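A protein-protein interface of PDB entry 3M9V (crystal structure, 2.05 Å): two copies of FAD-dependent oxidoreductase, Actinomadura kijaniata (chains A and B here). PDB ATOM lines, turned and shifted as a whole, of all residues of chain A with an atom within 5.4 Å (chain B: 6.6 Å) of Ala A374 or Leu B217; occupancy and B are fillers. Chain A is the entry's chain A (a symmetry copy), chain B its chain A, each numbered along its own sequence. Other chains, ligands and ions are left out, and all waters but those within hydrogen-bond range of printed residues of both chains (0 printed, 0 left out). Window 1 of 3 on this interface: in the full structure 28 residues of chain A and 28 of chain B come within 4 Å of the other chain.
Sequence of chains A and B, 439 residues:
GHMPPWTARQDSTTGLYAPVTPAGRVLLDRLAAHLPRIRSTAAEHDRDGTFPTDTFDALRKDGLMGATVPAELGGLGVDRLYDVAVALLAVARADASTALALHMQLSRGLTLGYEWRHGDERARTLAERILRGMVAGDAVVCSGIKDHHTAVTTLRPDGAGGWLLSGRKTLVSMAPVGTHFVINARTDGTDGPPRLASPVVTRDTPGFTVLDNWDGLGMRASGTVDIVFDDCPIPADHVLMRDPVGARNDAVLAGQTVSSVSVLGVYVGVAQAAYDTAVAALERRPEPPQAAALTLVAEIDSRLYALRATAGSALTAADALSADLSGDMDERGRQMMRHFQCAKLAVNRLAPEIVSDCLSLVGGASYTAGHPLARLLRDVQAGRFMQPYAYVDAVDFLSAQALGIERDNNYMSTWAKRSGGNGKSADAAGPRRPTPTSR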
ATOM      1  N   LEU A 359       3.606  26.645   2.954  1.00  0.00           N
ATOM      2  CA  LEU A 359       4.067  26.273   4.283  1.00  0.00           C
ATOM      3  C   LEU A 359       5.378  25.504   4.211  1.00  0.00           C
ATOM      4  O   LEU A 359       6.210  25.627   5.117  1.00  0.00           O
ATOM      5  CB  LEU A 359       3.018  25.411   4.996  1.00  0.00           C
ATOM      6  CG  LEU A 359       1.910  26.217   5.709  1.00  0.00           C
ATOM      7  CD1 LEU A 359       0.720  26.463   4.807  1.00  0.00           C
ATOM      8  CD2 LEU A 359       1.357  25.556   6.946  1.00  0.00           C
ATOM      9  N   SER A 366       5.449  28.529  10.197  1.00  0.00           N
ATOM     10  CA  SER A 366       4.088  28.623   9.688  1.00  0.00           C
ATOM     11  C   SER A 366       3.136  27.687  10.426  1.00  0.00           C
ATOM     12  O   SER A 366       1.919  27.773  10.218  1.00  0.00           O
ATOM     13  CB  SER A 366       4.116  28.300   8.193  1.00  0.00           C
ATOM     14  OG  SER A 366       4.382  26.916   8.026  1.00  0.00           O
ATOM     15  N   TYR A 367       3.649  26.804  11.292  1.00  0.00           N
ATOM     16  CA  TYR A 367       2.817  25.886  12.080  1.00  0.00           C
ATOM     17  C   TYR A 367       2.419  26.386  13.485  1.00  0.00           C
ATOM     18  O   TYR A 367       1.826  25.654  14.289  1.00  0.00           O
ATOM     19  CB  TYR A 367       3.466  24.497  12.151  1.00  0.00           C
ATOM     20  CG  TYR A 367       2.556  23.353  12.569  1.00  0.00           C
ATOM     21  CD1 TYR A 367       1.462  22.954  11.800  1.00  0.00           C
ATOM     22  CD2 TYR A 367       2.803  22.661  13.754  1.00  0.00           C
ATOM     23  CE1 TYR A 367       0.623  21.898  12.178  1.00  0.00           C
ATOM     24  CE2 TYR A 367       1.971  21.626  14.157  1.00  0.00           C
ATOM     25  CZ  TYR A 367       0.893  21.253  13.360  1.00  0.00           C
ATOM     26  OH  TYR A 367       0.114  20.208  13.765  1.00  0.00           O
ATOM     27  N   THR A 368       2.704  27.649  13.796  1.00  0.00           N
ATOM     28  CA  THR A 368       2.309  28.138  15.112  1.00  0.00           C
ATOM     29  C   THR A 368       1.040  28.912  14.823  1.00  0.00           C
ATOM     30  O   THR A 368       0.846  29.392  13.708  1.00  0.00           O
ATOM     31  CB  THR A 368       3.351  29.113  15.695  1.00  0.00           C
ATOM     32  OG1 THR A 368       3.375  30.238  14.820  1.00  0.00           O
ATOM     33  CG2 THR A 368       4.748  28.521  15.638  1.00  0.00           C
ATOM     34  N   ALA A 369       0.173  29.009  15.825  1.00  0.00           N
ATOM     35  CA  ALA A 369      -1.214  29.397  15.644  1.00  0.00           C
ATOM     36  C   ALA A 369      -1.345  30.808  15.092  1.00  0.00           C
ATOM     37  O   ALA A 369      -2.278  31.055  14.329  1.00  0.00           O
ATOM     38  CB  ALA A 369      -2.037  29.211  16.919  1.00  0.00           C
ATOM     39  N   GLY A 370      -0.417  31.693  15.441  1.00  0.00           N
ATOM     40  CA  GLY A 370      -0.492  33.085  15.015  1.00  0.00           C
ATOM     41  C   GLY A 370       0.071  33.397  13.630  1.00  0.00           C
ATOM     42  O   GLY A 370      -0.126  34.496  13.120  1.00  0.00           O
ATOM     43  N   HIS A 371       0.790  32.489  12.975  1.00  0.00           N
ATOM     44  CA  HIS A 371       1.381  32.862  11.697  1.00  0.00           C
ATOM     45  C   HIS A 371       0.243  32.986  10.688  1.00  0.00           C
ATOM     46  O   HIS A 371      -0.664  32.147  10.692  1.00  0.00           O
ATOM     47  CB  HIS A 371       2.366  31.773  11.240  1.00  0.00           C
ATOM     48  CG  HIS A 371       3.250  32.209  10.120  1.00  0.00           C
ATOM     49  ND1 HIS A 371       2.840  32.211   8.798  1.00  0.00           N
ATOM     50  CD2 HIS A 371       4.518  32.683  10.141  1.00  0.00           C
ATOM     51  CE1 HIS A 371       3.835  32.647   8.048  1.00  0.00           C
ATOM     52  NE2 HIS A 371       4.856  32.942   8.835  1.00  0.00           N
ATOM     53  N   PRO A 372       0.299  33.987   9.791  1.00  0.00           N
ATOM     54  CA  PRO A 372      -0.712  34.159   8.747  1.00  0.00           C
ATOM     55  C   PRO A 372      -0.967  32.915   7.898  1.00  0.00           C
ATOM     56  O   PRO A 372      -2.115  32.665   7.517  1.00  0.00           O
ATOM     57  CB  PRO A 372      -0.109  35.243   7.838  1.00  0.00           C
ATOM     58  CG  PRO A 372       0.807  36.000   8.739  1.00  0.00           C
ATOM     59  CD  PRO A 372       1.407  34.949   9.631  1.00  0.00           C
ATOM     60  N   LEU A 373       0.048  32.121   7.592  1.00  0.00           N
ATOM     61  CA  LEU A 373      -0.172  30.972   6.713  1.00  0.00           C
ATOM     62  C   LEU A 373      -1.094  29.942   7.381  1.00  0.00           C
ATOM     63  O   LEU A 373      -1.781  29.188   6.683  1.00  0.00           O
ATOM     64  CB  LEU A 373       1.127  30.275   6.300  1.00  0.00           C
ATOM     65  CG  LEU A 373       1.937  31.014   5.214  1.00  0.00           C
ATOM     66  CD1 LEU A 373       3.229  30.240   4.932  1.00  0.00           C
ATOM     67  CD2 LEU A 373       1.129  31.111   3.915  1.00  0.00           C
ATOM     68  N   ALA A 374      -1.060  29.892   8.714  1.00  0.00           N
ATOM     69  CA  ALA A 374      -1.784  28.897   9.486  1.00  0.00           C
ATOM     70  C   ALA A 374      -3.247  29.272   9.386  1.00  0.00           C
ATOM     71  O   ALA A 374      -4.115  28.403   9.295  1.00  0.00           O
ATOM     72  CB  ALA A 374      -1.325  28.936  10.936  1.00  0.00           C
ATOM     73  N   ARG A 375      -3.529  30.571   9.379  1.00  0.00           N
ATOM     74  CA  ARG A 375      -4.907  30.987   9.142  1.00  0.00           C
ATOM     75  C   ARG A 375      -5.369  30.778   7.687  1.00  0.00           C
ATOM     76  O   ARG A 375      -6.523  30.410   7.435  1.00  0.00           O
ATOM     77  CB  ARG A 375      -5.106  32.452   9.568  1.00  0.00           C
ATOM     78  CG  ARG A 375      -6.532  32.950   9.310  1.00  0.00           C
ATOM     79  CD  ARG A 375      -6.828  34.349   9.866  1.00  0.00           C
ATOM     80  NE  ARG A 375      -6.104  35.430   9.205  1.00  0.00           N
ATOM     81  CZ  ARG A 375      -5.001  36.011   9.671  1.00  0.00           C
ATOM     82  NH1 ARG A 375      -4.445  36.989   8.981  1.00  0.00           N
ATOM     83  NH2 ARG A 375      -4.401  35.623  10.789  1.00  0.00           N
ATOM     84  N   LEU A 376      -4.507  31.058   6.715  1.00  0.00           N
ATOM     85  CA  LEU A 376      -4.835  30.900   5.294  1.00  0.00           C
ATOM     86  C   LEU A 376      -5.088  29.421   5.003  1.00  0.00           C
ATOM     87  O   LEU A 376      -6.015  29.094   4.247  1.00  0.00           O
ATOM     88  CB  LEU A 376      -3.659  31.362   4.449  1.00  0.00           C
ATOM     89  CG  LEU A 376      -3.369  32.866   4.614  1.00  0.00           C
ATOM     90  CD1 LEU A 376      -2.485  33.373   3.480  1.00  0.00           C
ATOM     91  CD2 LEU A 376      -4.668  33.674   4.622  1.00  0.00           C
ATOM     92  N   LEU A 377      -4.330  28.538   5.655  1.00  0.00           N
ATOM     93  CA  LEU A 377      -4.621  27.123   5.448  1.00  0.00           C
ATOM     94  C   LEU A 377      -6.036  26.717   5.906  1.00  0.00           C
ATOM     95  O   LEU A 377      -6.703  25.863   5.295  1.00  0.00           O
ATOM     96  CB  LEU A 377      -3.574  26.254   6.148  1.00  0.00           C
ATOM     97  CG  LEU A 377      -3.802  24.737   5.985  1.00  0.00           C
ATOM     98  CD1 LEU A 377      -3.389  24.271   4.577  1.00  0.00           C
ATOM     99  CD2 LEU A 377      -2.972  23.922   6.981  1.00  0.00           C
ATOM    100  N   ARG A 378      -6.462  27.269   7.038  1.00  0.00           N
ATOM    101  CA  ARG A 378      -7.848  27.060   7.449  1.00  0.00           C
ATOM    102  C   ARG A 378      -8.866  27.764   6.562  1.00  0.00           C
ATOM    103  O   ARG A 378      -9.900  27.155   6.235  1.00  0.00           O
ATOM    104  CB  ARG A 378      -8.022  27.490   8.908  1.00  0.00           C
ATOM    105  CG  ARG A 378      -7.089  26.668   9.802  1.00  0.00           C
ATOM    106  CD  ARG A 378      -7.297  26.974  11.311  1.00  0.00           C
ATOM    107  NE  ARG A 378      -6.564  28.167  11.719  1.00  0.00           N
ATOM    108  CZ  ARG A 378      -7.131  29.363  11.909  1.00  0.00           C
ATOM    109  NH1 ARG A 378      -6.425  30.409  12.301  1.00  0.00           N
ATOM    110  NH2 ARG A 378      -8.436  29.554  11.769  1.00  0.00           N
ATOM    111  N   ASP B  46      -6.926  20.276  23.177  1.00  0.00           N
ATOM    112  CA  ASP B  46      -6.679  20.992  21.933  1.00  0.00           C
ATOM    113  C   ASP B  46      -7.227  22.413  21.963  1.00  0.00           C
ATOM    114  O   ASP B  46      -6.586  23.363  21.526  1.00  0.00           O
ATOM    115  CB  ASP B  46      -7.306  20.208  20.779  1.00  0.00           C
ATOM    116  CG  ASP B  46      -7.261  20.971  19.470  1.00  0.00           C
ATOM    117  OD1 ASP B  46      -6.200  21.171  18.851  1.00  0.00           O
ATOM    118  OD2 ASP B  46      -8.315  21.409  18.999  1.00  0.00           O
ATOM    119  N   TRP B 214       3.985  27.362  23.859  1.00  0.00           N
ATOM    120  CA  TRP B 214       3.601  26.606  22.671  1.00  0.00           C
ATOM    121  C   TRP B 214       2.172  26.942  22.273  1.00  0.00           C
ATOM    122  O   TRP B 214       1.228  26.707  23.018  1.00  0.00           O
ATOM    123  CB  TRP B 214       3.728  25.093  22.903  1.00  0.00           C
ATOM    124  CG  TRP B 214       3.190  24.235  21.791  1.00  0.00           C
ATOM    125  CD1 TRP B 214       2.186  23.314  21.900  1.00  0.00           C
ATOM    126  CD2 TRP B 214       3.581  24.239  20.405  1.00  0.00           C
ATOM    127  NE1 TRP B 214       1.931  22.747  20.680  1.00  0.00           N
ATOM    128  CE2 TRP B 214       2.773  23.278  19.742  1.00  0.00           C
ATOM    129  CE3 TRP B 214       4.522  24.960  19.666  1.00  0.00           C
ATOM    130  CZ2 TRP B 214       2.869  23.011  18.374  1.00  0.00           C
ATOM    131  CZ3 TRP B 214       4.639  24.680  18.298  1.00  0.00           C
ATOM    132  CH2 TRP B 214       3.818  23.713  17.677  1.00  0.00           C
ATOM    133  N   ASP B 215       2.019  27.429  21.050  1.00  0.00           N
ATOM    134  CA  ASP B 215       0.719  27.817  20.539  1.00  0.00           C
ATOM    135  C   ASP B 215       0.623  27.285  19.109  1.00  0.00           C
ATOM    136  O   ASP B 215       0.849  28.065  18.183  1.00  0.00           O
ATOM    137  CB  ASP B 215       0.599  29.350  20.568  1.00  0.00           C
ATOM    138  CG  ASP B 215      -0.848  29.806  20.431  1.00  0.00           C
ATOM    139  OD1 ASP B 215      -1.783  29.004  20.657  1.00  0.00           O
ATOM    140  OD2 ASP B 215      -1.076  30.963  20.032  1.00  0.00           O
ATOM    141  N   GLY B 216       0.274  26.007  18.938  1.00  0.00           N
ATOM    142  CA  GLY B 216       0.447  25.292  17.667  1.00  0.00           C
ATOM    143  C   GLY B 216      -0.803  25.445  16.812  1.00  0.00           C
ATOM    144  O   GLY B 216      -1.885  25.671  17.336  1.00  0.00           O
ATOM    145  N   LEU B 217      -0.688  25.305  15.498  1.00  0.00           N
ATOM    146  CA  LEU B 217      -1.886  25.225  14.663  1.00  0.00           C
ATOM    147  C   LEU B 217      -2.494  23.873  15.052  1.00  0.00           C
ATOM    148  O   LEU B 217      -3.687  23.779  15.358  1.00  0.00           O
ATOM    149  CB  LEU B 217      -1.479  25.276  13.188  1.00  0.00           C
ATOM    150  CG  LEU B 217      -2.555  24.867  12.168  1.00  0.00           C
ATOM    151  CD1 LEU B 217      -3.834  25.710  12.210  1.00  0.00           C
ATOM    152  CD2 LEU B 217      -1.930  24.773  10.790  1.00  0.00           C
ATOM    153  N   GLY B 218      -1.662  22.826  15.082  1.00  0.00           N
ATOM    154  CA  GLY B 218      -2.035  21.522  15.647  1.00  0.00           C
ATOM    155  C   GLY B 218      -1.034  21.026  16.687  1.00  0.00           C
ATOM    156  O   GLY B 218      -0.146  21.792  17.076  1.00  0.00           O
ATOM    157  N   MET B 219      -1.137  19.756  17.096  1.00  0.00           N
ATOM    158  CA  MET B 219      -0.331  19.162  18.175  1.00  0.00           C
ATOM    159  C   MET B 219      -0.420  20.095  19.397  1.00  0.00           C
ATOM    160  O   MET B 219       0.555  20.310  20.131  1.00  0.00           O
ATOM    161  CB  MET B 219       1.135  18.893  17.782  1.00  0.00           C
ATOM    162  CG  MET B 219       1.359  17.865  16.641  1.00  0.00           C
ATOM    163  SD  MET B 219       0.486  16.306  17.024  1.00  0.00           S
ATOM    164  CE  MET B 219       0.930  15.312  15.597  1.00  0.00           C
ATOM    165  N   ARG B 220      -1.611  20.651  19.594  1.00  0.00           N
ATOM    166  CA  ARG B 220      -1.766  21.725  20.561  1.00  0.00           C
ATOM    167  C   ARG B 220      -1.514  21.297  21.999  1.00  0.00           C
ATOM    168  O   ARG B 220      -1.096  22.115  22.826  1.00  0.00           O
ATOM    169  CB  ARG B 220      -3.085  22.481  20.360  1.00  0.00           C
ATOM    170  CG  ARG B 220      -3.010  23.394  19.153  1.00  0.00           C
ATOM    171  CD  ARG B 220      -4.364  24.080  18.901  1.00  0.00           C
ATOM    172  NE  ARG B 220      -4.780  24.832  20.081  1.00  0.00           N
ATOM    173  CZ  ARG B 220      -4.270  25.994  20.486  1.00  0.00           C
ATOM    174  NH1 ARG B 220      -3.310  26.631  19.816  1.00  0.00           N
ATOM    175  NH2 ARG B 220      -4.749  26.530  21.602  1.00  0.00           N
ATOM    176  N   ARG B 375      -9.668  18.884  13.701  1.00  0.00           N
ATOM    177  CA  ARG B 375      -8.430  18.735  14.460  1.00  0.00           C
ATOM    178  C   ARG B 375      -7.387  17.842  13.762  1.00  0.00           C
ATOM    179  O   ARG B 375      -6.181  18.111  13.822  1.00  0.00           O
ATOM    180  CB  ARG B 375      -8.729  18.212  15.877  1.00  0.00           C
ATOM    181  CG  ARG B 375      -7.458  18.007  16.707  1.00  0.00           C
ATOM    182  CD  ARG B 375      -7.709  17.645  18.177  1.00  0.00           C
ATOM    183  NE  ARG B 375      -8.310  16.331  18.383  1.00  0.00           N
ATOM    184  CZ  ARG B 375      -9.602  16.107  18.614  1.00  0.00           C
ATOM    185  NH1 ARG B 375     -10.020  14.869  18.795  1.00  0.00           N
ATOM    186  NH2 ARG B 375     -10.509  17.076  18.631  1.00  0.00           N
ATOM    187  N   LEU B 377      -7.026  17.429  10.612  1.00  0.00           N
ATOM    188  CA  LEU B 377      -6.390  18.190   9.541  1.00  0.00           C
ATOM    189  C   LEU B 377      -5.231  19.081  10.031  1.00  0.00           C
ATOM    190  O   LEU B 377      -4.212  19.270   9.342  1.00  0.00           O
ATOM    191  CB  LEU B 377      -7.426  19.039   8.800  1.00  0.00           C
ATOM    192  CG  LEU B 377      -6.843  19.882   7.648  1.00  0.00           C
ATOM    193  CD1 LEU B 377      -6.544  19.001   6.422  1.00  0.00           C
ATOM    194  CD2 LEU B 377      -7.816  20.969   7.184  1.00  0.00           C
ATOM    195  N   ARG B 378      -5.424  19.703  11.191  1.00  0.00           N
ATOM    196  CA  ARG B 378      -4.313  20.431  11.796  1.00  0.00           C
ATOM    197  C   ARG B 378      -3.193  19.535  12.306  1.00  0.00           C
ATOM    198  O   ARG B 378      -2.014  19.868  12.095  1.00  0.00           O
ATOM    199  CB  ARG B 378      -4.837  21.325  12.924  1.00  0.00           C
ATOM    200  CG  ARG B 378      -5.860  22.317  12.360  1.00  0.00           C
ATOM    201  CD  ARG B 378      -6.349  23.331  13.432  1.00  0.00           C
ATOM    202  NE  ARG B 378      -7.414  22.767  14.253  1.00  0.00           N
ATOM    203  CZ  ARG B 378      -7.233  22.304  15.494  1.00  0.00           C
ATOM    204  NH1 ARG B 378      -8.237  21.822  16.206  1.00  0.00           N
ATOM    205  NH2 ARG B 378      -6.054  22.351  16.099  1.00  0.00           N
ATOM    206  N   ASP B 379      -3.529  18.474  13.040  1.00  0.00           N
ATOM    207  CA  ASP B 379      -2.434  17.683  13.616  1.00  0.00           C
ATOM    208  C   ASP B 379      -1.622  16.980  12.528  1.00  0.00           C
ATOM    209  O   ASP B 379      -0.418  16.740  12.684  1.00  0.00           O
ATOM    210  CB  ASP B 379      -2.930  16.574  14.552  1.00  0.00           C
ATOM    211  CG  ASP B 379      -3.549  17.142  15.802  1.00  0.00           C
ATOM    212  OD1 ASP B 379      -3.350  18.334  16.076  1.00  0.00           O
ATOM    213  OD2 ASP B 379      -4.254  16.386  16.479  1.00  0.00           O
ATOM    214  N   GLN B 381      -0.455  17.839   9.832  1.00  0.00           N
ATOM    215  CA  GLN B 381       0.548  18.654   9.141  1.00  0.00           C
ATOM    216  C   GLN B 381       1.893  18.673   9.875  1.00  0.00           C
ATOM    217  O   GLN B 381       2.902  19.015   9.262  1.00  0.00           O
ATOM    218  CB  GLN B 381       0.064  20.095   8.910  1.00  0.00           C
ATOM    219  CG  GLN B 381      -1.375  20.258   8.349  1.00  0.00           C
ATOM    220  CD  GLN B 381      -1.530  19.721   6.934  1.00  0.00           C
ATOM    221  OE1 GLN B 381      -0.557  19.611   6.177  1.00  0.00           O
ATOM    222  NE2 GLN B 381      -2.747  19.313   6.593  1.00  0.00           N
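The backbone NH of Leu B217 sits at hydrogen-bond distance from the backbone carbonyl oxygen of Tyr A367. The side-chain hydroxyl (OH) of Tyr A367 sits close to the backbone NH (N) of Gly B218 (3.4 Å). The backbone carbonyl oxygen (O) of Arg B378 lies within hydrogen-bond range of the side-chain hydroxyl (OH) of Tyr A367 (2.7 Å). N of Ala A369 lies within hydrogen-bond range of O of Asp B215, 2.6 Å away.
The side-chain carboxylate (OD1) of Asp B215 lies within salt-bridge range of the guanidinium group (NH1) of Arg B220 (2.9 Å). The backbone carbonyl oxygen of Ala A374 sits at hydrogen-bond distance from the guanidinium group of Arg A378 (3.5 Å). The side-chain amide nitrogen (NE2) of Gln B381 is in hydrogen-bond range of the backbone carbonyl oxygen (O) of Leu B377 (3.1 Å). The backbone NH (N) of Met B219 is in hydrogen-bond range of the side-chain carboxylate (OD1) of Asp B379 (2.8 Å). O of Met B219 is in hydrogen-bond range of NE1 of Trp B214 (2.9 Å). O of Gly B216 lies within hydrogen-bond range of NH1 of Arg B220 (3.0 Å).
Among the printed residues, pairs that only touch across the chains: Tyr A367 with Gly B216 (3.6 Å), Tyr A367 with Met B219 (3.6 Å), Tyr A367 with Asp B379 (3.6 Å), Tyr A367 with Gln B381 (3.8 Å), Thr A368 with Asp B215 (3.4 Å), Ala A369 with Gly B216 (3.6 Å), Ala A369 with Leu B217 (3.8 Å), Ala A374 with Leu B217 (3.98 Å) and Arg A378 with Leu B217 (3.7 Å).
Printed residues of chain B within 4 Å of Tyr A367: Gly B216 (3.6 Å), Leu B217 (2.8 Å), Gly B218 (3.1 Å), Met B219 (3.6 Å), Arg B378 (2.7 Å), Asp B379 (3.6 Å) and Gln B381 (3.8 Å). Of the printed residues of chain B, Thr A368 touches Asp B215 (3.4 Å). Of the printed residues of chain B, Ala A374 touches Leu B217 (3.98 Å). Printed residues of chain A within 4 Å of Gly B216: Tyr A367 (3.6 Å) and Ala A369 (3.6 Å). Printed residues of chain A within 4 Å of Asp B379: Tyr A367 (3.6 Å). Printed residues of chain A within 4 Å of Gln B381: Tyr A367 (3.8 Å). The nearest printed residue of chain B that does not touch Ala A374 is Gly B216 (6.9 Å). The nearest printed residue of chain A that does not touch Asp B215 is Tyr A367 (4.7 Å).
Hydrophobic or aromatic side chains of chain B that line the printed part of chain A: Leu B217 and Met B219. Hydrophobic or aromatic side chains of chain A that line the printed part of chain B: Tyr A367 and Ala A369.
Positions printed for both chains: 375, 377 and 378.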
